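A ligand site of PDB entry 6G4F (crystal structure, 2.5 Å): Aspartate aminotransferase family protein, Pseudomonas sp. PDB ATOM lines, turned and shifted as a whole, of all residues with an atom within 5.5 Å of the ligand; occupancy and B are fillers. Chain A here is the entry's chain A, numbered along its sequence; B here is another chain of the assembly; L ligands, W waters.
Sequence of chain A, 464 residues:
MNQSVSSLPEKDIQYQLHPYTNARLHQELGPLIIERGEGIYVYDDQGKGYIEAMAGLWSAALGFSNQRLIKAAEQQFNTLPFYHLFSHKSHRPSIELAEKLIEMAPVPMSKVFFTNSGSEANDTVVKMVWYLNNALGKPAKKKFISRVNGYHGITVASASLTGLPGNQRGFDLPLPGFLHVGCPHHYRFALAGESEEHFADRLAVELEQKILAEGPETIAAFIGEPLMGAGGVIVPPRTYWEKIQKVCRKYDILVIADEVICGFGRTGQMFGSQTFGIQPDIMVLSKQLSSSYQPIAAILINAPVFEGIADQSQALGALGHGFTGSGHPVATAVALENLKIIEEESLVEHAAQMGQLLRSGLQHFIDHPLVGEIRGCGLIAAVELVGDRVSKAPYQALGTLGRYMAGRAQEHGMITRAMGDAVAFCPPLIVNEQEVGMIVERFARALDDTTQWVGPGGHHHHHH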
ATOM      1  N   TRP A  58      26.784 -12.101 -35.314  1.00  0.00           N
ATOM      2  CA  TRP A  58      27.593 -13.055 -36.052  1.00  0.00           C
ATOM      3  C   TRP A  58      26.788 -13.762 -37.126  1.00  0.00           C
ATOM      4  O   TRP A  58      27.147 -14.861 -37.499  1.00  0.00           O
ATOM      5  CB  TRP A  58      28.143 -14.130 -35.100  1.00  0.00           C
ATOM      6  CG  TRP A  58      28.583 -13.687 -33.730  1.00  0.00           C
ATOM      7  CD1 TRP A  58      27.802 -13.526 -32.627  1.00  0.00           C
ATOM      8  CD2 TRP A  58      29.926 -13.428 -33.312  1.00  0.00           C
ATOM      9  NE1 TRP A  58      28.575 -13.149 -31.554  1.00  0.00           N
ATOM     10  CE2 TRP A  58      29.885 -13.105 -31.948  1.00  0.00           C
ATOM     11  CE3 TRP A  58      31.174 -13.454 -33.962  1.00  0.00           C
ATOM     12  CZ2 TRP A  58      31.030 -12.787 -31.220  1.00  0.00           C
ATOM     13  CZ3 TRP A  58      32.318 -13.145 -33.230  1.00  0.00           C
ATOM     14  CH2 TRP A  58      32.227 -12.807 -31.883  1.00  0.00           C
ATOM     15  N   ASN A 116      14.098 -23.480 -32.897  1.00  0.00           N
ATOM     16  CA  ASN A 116      14.127 -22.043 -33.144  1.00  0.00           C
ATOM     17  C   ASN A 116      15.508 -21.477 -32.893  1.00  0.00           C
ATOM     18  O   ASN A 116      15.973 -20.653 -33.663  1.00  0.00           O
ATOM     19  CB  ASN A 116      13.107 -21.310 -32.276  1.00  0.00           C
ATOM     20  CG  ASN A 116      11.705 -21.876 -32.402  1.00  0.00           C
ATOM     21  OD1 ASN A 116      11.052 -21.749 -33.446  1.00  0.00           O
ATOM     22  ND2 ASN A 116      11.231 -22.520 -31.345  1.00  0.00           N
ATOM     23  N   SER A 117      16.163 -21.890 -31.811  1.00  0.00           N
ATOM     24  CA  SER A 117      17.419 -21.276 -31.433  1.00  0.00           C
ATOM     25  C   SER A 117      18.560 -22.257 -31.269  1.00  0.00           C
ATOM     26  O   SER A 117      18.355 -23.464 -31.151  1.00  0.00           O
ATOM     27  CB  SER A 117      17.249 -20.521 -30.118  1.00  0.00           C
ATOM     28  OG  SER A 117      16.901 -21.435 -29.113  1.00  0.00           O
ATOM     29  N   GLY A 118      19.764 -21.707 -31.243  1.00  0.00           N
ATOM     30  CA  GLY A 118      20.947 -22.484 -30.955  1.00  0.00           C
ATOM     31  C   GLY A 118      20.874 -23.036 -29.546  1.00  0.00           C
ATOM     32  O   GLY A 118      21.231 -24.184 -29.319  1.00  0.00           O
ATOM     33  N   SER A 119      20.405 -22.221 -28.611  1.00  0.00           N
ATOM     34  CA  SER A 119      20.292 -22.653 -27.236  1.00  0.00           C
ATOM     35  C   SER A 119      19.345 -23.829 -27.148  1.00  0.00           C
ATOM     36  O   SER A 119      19.654 -24.817 -26.506  1.00  0.00           O
ATOM     37  CB  SER A 119      19.828 -21.501 -26.352  1.00  0.00           C
ATOM     38  OG  SER A 119      20.751 -20.430 -26.381  1.00  0.00           O
ATOM     39  N   GLU A 120      18.199 -23.742 -27.782  1.00  0.00           N
ATOM     40  CA  GLU A 120      17.282 -24.864 -27.845  1.00  0.00           C
ATOM     41  C   GLU A 120      17.931 -26.085 -28.515  1.00  0.00           C
ATOM     42  O   GLU A 120      17.659 -27.218 -28.137  1.00  0.00           O
ATOM     43  CB  GLU A 120      16.061 -24.506 -28.674  1.00  0.00           C
ATOM     44  CG  GLU A 120      14.973 -23.674 -28.000  1.00  0.00           C
ATOM     45  CD  GLU A 120      13.907 -23.246 -29.009  1.00  0.00           C
ATOM     46  OE1 GLU A 120      14.173 -23.356 -30.225  1.00  0.00           O
ATOM     47  OE2 GLU A 120      12.817 -22.801 -28.586  1.00  0.00           O
ATOM     48  N   ASN A 122      21.211 -27.046 -28.719  1.00  0.00           N
ATOM     49  CA  ASN A 122      22.159 -27.725 -27.841  1.00  0.00           C
ATOM     50  C   ASN A 122      21.442 -28.354 -26.639  1.00  0.00           C
ATOM     51  O   ASN A 122      21.819 -29.435 -26.185  1.00  0.00           O
ATOM     52  CB  ASN A 122      23.278 -26.775 -27.377  1.00  0.00           C
ATOM     53  CG  ASN A 122      24.304 -26.494 -28.474  1.00  0.00           C
ATOM     54  OD1 ASN A 122      24.610 -27.369 -29.275  1.00  0.00           O
ATOM     55  ND2 ASN A 122      24.835 -25.293 -28.510  1.00  0.00           N
ATOM     56  N   TYR A 151      30.901 -20.931 -25.813  1.00  0.00           N
ATOM     57  CA  TYR A 151      29.537 -20.452 -25.672  1.00  0.00           C
ATOM     58  C   TYR A 151      28.624 -21.375 -26.478  1.00  0.00           C
ATOM     59  O   TYR A 151      28.885 -21.645 -27.632  1.00  0.00           O
ATOM     60  CB  TYR A 151      29.398 -19.013 -26.151  1.00  0.00           C
ATOM     61  CG  TYR A 151      28.021 -18.431 -25.926  1.00  0.00           C
ATOM     62  CD1 TYR A 151      27.671 -17.884 -24.706  1.00  0.00           C
ATOM     63  CD2 TYR A 151      27.069 -18.457 -26.927  1.00  0.00           C
ATOM     64  CE1 TYR A 151      26.405 -17.377 -24.490  1.00  0.00           C
ATOM     65  CE2 TYR A 151      25.807 -17.946 -26.723  1.00  0.00           C
ATOM     66  CZ  TYR A 151      25.470 -17.402 -25.509  1.00  0.00           C
ATOM     67  OH  TYR A 151      24.206 -16.910 -25.320  1.00  0.00           O
ATOM     68  N   HIS A 152      27.575 -21.883 -25.839  1.00  0.00           N
ATOM     69  CA  HIS A 152      26.652 -22.829 -26.477  1.00  0.00           C
ATOM     70  C   HIS A 152      25.187 -22.521 -26.174  1.00  0.00           C
ATOM     71  O   HIS A 152      24.326 -23.376 -26.372  1.00  0.00           O
ATOM     72  CB  HIS A 152      26.967 -24.273 -26.043  1.00  0.00           C
ATOM     73  CG  HIS A 152      28.368 -24.701 -26.319  1.00  0.00           C
ATOM     74  ND1 HIS A 152      28.827 -24.960 -27.591  1.00  0.00           N
ATOM     75  CD2 HIS A 152      29.422 -24.892 -25.483  1.00  0.00           C
ATOM     76  CE1 HIS A 152      30.101 -25.303 -27.528  1.00  0.00           C
ATOM     77  NE2 HIS A 152      30.485 -25.274 -26.270  1.00  0.00           N
ATOM     78  N   GLY A 153      24.901 -21.303 -25.726  1.00  0.00           N
ATOM     79  CA  GLY A 153      23.517 -20.924 -25.477  1.00  0.00           C
ATOM     80  C   GLY A 153      23.263 -20.755 -24.007  1.00  0.00           C
ATOM     81  O   GLY A 153      24.178 -20.900 -23.195  1.00  0.00           O
ATOM     82  N   ILE A 154      22.022 -20.446 -23.671  1.00  0.00           N
ATOM     83  CA  ILE A 154      21.715 -19.931 -22.342  1.00  0.00           C
ATOM     84  C   ILE A 154      20.458 -20.502 -21.720  1.00  0.00           C
ATOM     85  O   ILE A 154      19.865 -19.870 -20.834  1.00  0.00           O
ATOM     86  CB  ILE A 154      21.714 -18.381 -22.299  1.00  0.00           C
ATOM     87  CG1 ILE A 154      21.071 -17.772 -23.544  1.00  0.00           C
ATOM     88  CG2 ILE A 154      23.148 -17.856 -22.185  1.00  0.00           C
ATOM     89  CD1 ILE A 154      19.573 -17.934 -23.581  1.00  0.00           C
ATOM     90  N   GLU A 225      32.830 -25.544 -30.294  1.00  0.00           N
ATOM     91  CA  GLU A 225      32.815 -24.701 -31.487  1.00  0.00           C
ATOM     92  C   GLU A 225      34.155 -24.932 -32.154  1.00  0.00           C
ATOM     93  O   GLU A 225      35.191 -24.968 -31.473  1.00  0.00           O
ATOM     94  CB  GLU A 225      32.696 -23.225 -31.123  1.00  0.00           C
ATOM     95  CG  GLU A 225      31.546 -22.829 -30.210  1.00  0.00           C
ATOM     96  CD  GLU A 225      31.804 -21.505 -29.527  1.00  0.00           C
ATOM     97  OE1 GLU A 225      31.635 -20.476 -30.194  1.00  0.00           O
ATOM     98  OE2 GLU A 225      32.195 -21.493 -28.343  1.00  0.00           O
ATOM     99  N   ALA A 230      31.917 -16.187 -29.277  1.00  0.00           N
ATOM    100  CA  ALA A 230      31.628 -15.196 -28.265  1.00  0.00           C
ATOM    101  C   ALA A 230      32.710 -15.107 -27.206  1.00  0.00           C
ATOM    102  O   ALA A 230      32.860 -14.077 -26.566  1.00  0.00           O
ATOM    103  CB  ALA A 230      30.283 -15.488 -27.615  1.00  0.00           C
ATOM    104  N   ASP A 258      29.611 -27.501 -32.534  1.00  0.00           N
ATOM    105  CA  ASP A 258      28.670 -26.369 -32.477  1.00  0.00           C
ATOM    106  C   ASP A 258      29.071 -25.396 -33.540  1.00  0.00           C
ATOM    107  O   ASP A 258      30.003 -24.633 -33.382  1.00  0.00           O
ATOM    108  CB  ASP A 258      28.697 -25.691 -31.108  1.00  0.00           C
ATOM    109  CG  ASP A 258      27.652 -24.588 -30.981  1.00  0.00           C
ATOM    110  OD1 ASP A 258      27.237 -24.061 -32.036  1.00  0.00           O
ATOM    111  OD2 ASP A 258      27.252 -24.238 -29.833  1.00  0.00           O
ATOM    112  N   VAL A 260      27.080 -23.021 -34.875  1.00  0.00           N
ATOM    113  CA  VAL A 260      26.123 -21.929 -34.912  1.00  0.00           C
ATOM    114  C   VAL A 260      26.747 -20.675 -35.535  1.00  0.00           C
ATOM    115  O   VAL A 260      26.108 -19.996 -36.318  1.00  0.00           O
ATOM    116  CB  VAL A 260      25.542 -21.679 -33.492  1.00  0.00           C
ATOM    117  CG1 VAL A 260      24.969 -20.271 -33.333  1.00  0.00           C
ATOM    118  CG2 VAL A 260      24.474 -22.726 -33.173  1.00  0.00           C
ATOM    119  N   ILE A 261      28.006 -20.394 -35.227  1.00  0.00           N
ATOM    120  CA  ILE A 261      28.680 -19.246 -35.856  1.00  0.00           C
ATOM    121  C   ILE A 261      29.489 -19.629 -37.092  1.00  0.00           C
ATOM    122  O   ILE A 261      29.396 -18.975 -38.153  1.00  0.00           O
ATOM    123  CB  ILE A 261      29.589 -18.511 -34.851  1.00  0.00           C
ATOM    124  CG1 ILE A 261      28.731 -17.683 -33.906  1.00  0.00           C
ATOM    125  CG2 ILE A 261      30.612 -17.622 -35.566  1.00  0.00           C
ATOM    126  CD1 ILE A 261      29.493 -16.971 -32.804  1.00  0.00           C
ATOM    127  N   SER A 286      22.782 -22.599 -36.905  1.00  0.00           N
ATOM    128  CA  SER A 286      21.836 -21.506 -36.815  1.00  0.00           C
ATOM    129  C   SER A 286      22.417 -20.279 -37.491  1.00  0.00           C
ATOM    130  O   SER A 286      23.235 -20.414 -38.398  1.00  0.00           O
ATOM    131  CB  SER A 286      21.487 -21.193 -35.356  1.00  0.00           C
ATOM    132  OG  SER A 286      20.232 -20.552 -35.270  1.00  0.00           O
ATOM    133  N   LYS A 287      21.965 -19.096 -37.070  1.00  0.00           N
ATOM    134  CA  LYS A 287      22.533 -17.820 -37.510  1.00  0.00           C
ATOM    135  C   LYS A 287      22.621 -17.725 -39.026  1.00  0.00           C
ATOM    136  O   LYS A 287      21.629 -17.422 -39.653  1.00  0.00           O
ATOM    137  CB  LYS A 287      23.867 -17.543 -36.851  1.00  0.00           C
ATOM    138  CG  LYS A 287      23.733 -17.229 -35.362  1.00  0.00           C
ATOM    139  CD  LYS A 287      25.107 -17.130 -34.672  1.00  0.00           C
ATOM    140  CE  LYS A 287      24.947 -16.861 -33.181  1.00  0.00           C
ATOM    141  NZ  LYS A 287      24.525 -15.463 -32.890  1.00  0.00           N
ATOM    142  N   ASN B 116      11.993 -16.895 -28.315  1.00  0.00           N
ATOM    143  CA  ASN B 116      11.414 -17.509 -29.503  1.00  0.00           C
ATOM    144  C   ASN B 116      10.288 -18.443 -29.125  1.00  0.00           C
ATOM    145  O   ASN B 116       9.259 -18.441 -29.784  1.00  0.00           O
ATOM    146  CB  ASN B 116      12.460 -18.274 -30.305  1.00  0.00           C
ATOM    147  CG  ASN B 116      13.656 -17.420 -30.659  1.00  0.00           C
ATOM    148  OD1 ASN B 116      13.563 -16.516 -31.491  1.00  0.00           O
ATOM    149  ND2 ASN B 116      14.780 -17.690 -30.029  1.00  0.00           N
ATOM    150  N   GLU B 120      11.610 -21.968 -24.157  1.00  0.00           N
ATOM    151  CA  GLU B 120      12.626 -21.008 -23.804  1.00  0.00           C
ATOM    152  C   GLU B 120      12.133 -20.009 -22.761  1.00  0.00           C
ATOM    153  O   GLU B 120      12.893 -19.566 -21.902  1.00  0.00           O
ATOM    154  CB  GLU B 120      13.033 -20.194 -25.032  1.00  0.00           C
ATOM    155  CG  GLU B 120      13.990 -20.838 -26.012  1.00  0.00           C
ATOM    156  CD  GLU B 120      14.157 -19.968 -27.252  1.00  0.00           C
ATOM    157  OE1 GLU B 120      13.315 -19.047 -27.451  1.00  0.00           O
ATOM    158  OE2 GLU B 120      15.119 -20.179 -28.043  1.00  0.00           O
ATOM    159  N   GLY B 322      20.077 -14.045 -22.909  1.00  0.00           N
ATOM    160  CA  GLY B 322      19.484 -13.544 -24.122  1.00  0.00           C
ATOM    161  C   GLY B 322      19.659 -14.467 -25.305  1.00  0.00           C
ATOM    162  O   GLY B 322      20.706 -15.049 -25.500  1.00  0.00           O
ATOM    163  N   PHE B 323      18.611 -14.585 -26.102  1.00  0.00           N
ATOM    164  CA  PHE B 323      18.658 -15.348 -27.331  1.00  0.00           C
ATOM    165  C   PHE B 323      18.875 -14.416 -28.498  1.00  0.00           C
ATOM    166  O   PHE B 323      18.405 -13.285 -28.508  1.00  0.00           O
ATOM    167  CB  PHE B 323      17.337 -16.078 -27.526  1.00  0.00           C
ATOM    168  CG  PHE B 323      16.979 -16.982 -26.398  1.00  0.00           C
ATOM    169  CD1 PHE B 323      17.448 -18.284 -26.367  1.00  0.00           C
ATOM    170  CD2 PHE B 323      16.156 -16.533 -25.374  1.00  0.00           C
ATOM    171  CE1 PHE B 323      17.090 -19.126 -25.333  1.00  0.00           C
ATOM    172  CE2 PHE B 323      15.822 -17.375 -24.319  1.00  0.00           C
ATOM    173  CZ  PHE B 323      16.286 -18.666 -24.308  1.00  0.00           C
ATOM    174  N   THR B 324      19.599 -14.913 -29.488  1.00  0.00           N
ATOM    175  CA  THR B 324      19.827 -14.199 -30.738  1.00  0.00           C
ATOM    176  C   THR B 324      18.509 -13.612 -31.296  1.00  0.00           C
ATOM    177  O   THR B 324      18.449 -12.445 -31.687  1.00  0.00           O
ATOM    178  CB  THR B 324      20.514 -15.141 -31.753  1.00  0.00           C
ATOM    179  OG1 THR B 324      21.835 -15.452 -31.274  1.00  0.00           O
ATOM    180  CG2 THR B 324      20.651 -14.496 -33.113  1.00  0.00           C
ATOM    181  N   GLY B 325      17.462 -14.417 -31.284  1.00  0.00           N
ATOM    182  CA  GLY B 325      16.162 -14.032 -31.795  1.00  0.00           C
ATOM    183  C   GLY B 325      15.255 -13.317 -30.809  1.00  0.00           C
ATOM    184  O   GLY B 325      14.081 -13.081 -31.148  1.00  0.00           O
HETATM  185  N1  LIG L   1      26.185 -21.624 -30.028  1.00  0.00           N
HETATM  186  C1  LIG L   1      27.010 -20.624 -30.400  1.00  0.00           C
HETATM  187  C2  LIG L   1      28.403 -20.912 -30.879  1.00  0.00           C
HETATM  188  C3  LIG L   1      26.540 -19.231 -30.347  1.00  0.00           C
HETATM  189  O1  LIG L   1      27.388 -18.241 -30.717  1.00  0.00           O
HETATM  190  C4  LIG L   1      25.167 -18.972 -29.881  1.00  0.00           C
HETATM  191  C5  LIG L   1      24.531 -17.605 -29.799  1.00  0.00           C
HETATM  192  N2  LIG L   1      25.467 -16.524 -29.998  1.00  0.00           N
HETATM  193  C6  LIG L   1      24.376 -20.147 -29.494  1.00  0.00           C
HETATM  194  C7  LIG L   1      24.936 -21.426 -29.584  1.00  0.00           C
HETATM  195  C8  LIG L   1      22.951 -19.953 -29.001  1.00  0.00           C
HETATM  196  O2  LIG L   1      22.154 -19.329 -30.016  1.00  0.00           O
HETATM  197  P1  LIG L   1      20.751 -18.615 -29.716  1.00  0.00           P
HETATM  198  O3  LIG L   1      21.246 -17.231 -29.418  1.00  0.00           O
HETATM  199  O4  LIG L   1      20.083 -19.402 -28.614  1.00  0.00           O
HETATM  200  O5  LIG L   1      19.995 -18.781 -31.008  1.00  0.00           O
HETATM  201  O   HOH W   1      29.819 -18.307 -29.436  1.00  0.00           O
HETATM  202  O   HOH W   2      22.355 -16.590 -27.055  1.00  0.00           O
HETATM  203  O   HOH W   3      20.135 -18.182 -33.623  1.00  0.00           O
HETATM  204  O   HOH W   4      17.703 -17.240 -30.814  1.00  0.00           O
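N1 of the ligand sits at hydrogen-bond distance from OD2 of Asp 258 (2.8 Å). The side-chain hydroxyl (OG) of Ser 119 lies within hydrogen-bond range of an oxygen (O4) of the ligand. OG1 of Thr 324 of chain B is in hydrogen-bond range of O3 of the ligand, at 2.6 Å. The side-chain amino group of Lys 287 lies close to a nitrogen (N2) of the ligand, at 3.2 Å. N of Gly 118 is in hydrogen-bond range of O5 of the ligand, at 2.9 Å. N of Ser 119 lies within hydrogen-bond range of O4 of the ligand, at 2.8 Å. N of Thr 324 of chain B lies within hydrogen-bond range of O3 of the ligand, 2.8 Å away.
The side-chain carboxylate (OD2) of Asp 258 is in hydrogen-bond range of the side-chain amide nitrogen (ND2) of Asn 122. OD1 of Asp 258 lies within hydrogen-bond range of N of Val 260. OE2 of Glu 225 lies within hydrogen-bond range of N of Tyr 151 (2.9 Å). The side-chain amide nitrogen of Asn 122 lies within hydrogen-bond range of the backbone carbonyl oxygen of His 152, at 2.9 Å. The backbone NH of Ser 117 lies within hydrogen-bond range of the side-chain carboxylate of Glu 120 of chain A, at 2.9 Å. OG1 of Thr 324 of chain B sits at hydrogen-bond distance from NZ of Lys 287 (3.1 Å). OG of Ser 119 is in hydrogen-bond range of N of Ile 154, at 3.0 Å. The side-chain carboxylate of Asp 258 sits at hydrogen-bond distance from a ring nitrogen (ND1) of His 152, at 2.8 Å.
Merely in contact with the ligand: Ile 261 (3.2 Å), Glu 225 (3.3 Å), Tyr 151 (3.3 Å), Ser 117 (3.4 Å), Val 260 (3.5 Å), His 152 (3.6 Å), Phe 323 of chain B (3.6 Å) and Gly 153 (3.7 Å). Hydrophobic or aromatic side chains that line the ligand: Tyr 151, Val 260, Ile 261 and Phe 323 of chain B. Of the 24 residues printed, 13 come within 4 Å of the ligand. Along chain A the residues within 4 Å of the ligand span positions 117 to 287. The nearest printed residue that does not touch the ligand is Asn 122 (4.01 Å).
Water W3 bridges an oxygen (O5) of the ligand (2.7 Å) and the side-chain hydroxyl (OG) of Ser 286 (2.9 Å). Water W2 lies within hydrogen-bond range of the side-chain hydroxyl of Tyr 151, an oxygen (O3) of the ligand and the backbone carbonyl oxygen of Gly 322 of chain B. Water W1 lies within hydrogen-bond range of O1 of the ligand (2.7 Å), OE1 of Glu 225 (2.9 Å) and N of Ala 230 (3.0 Å).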
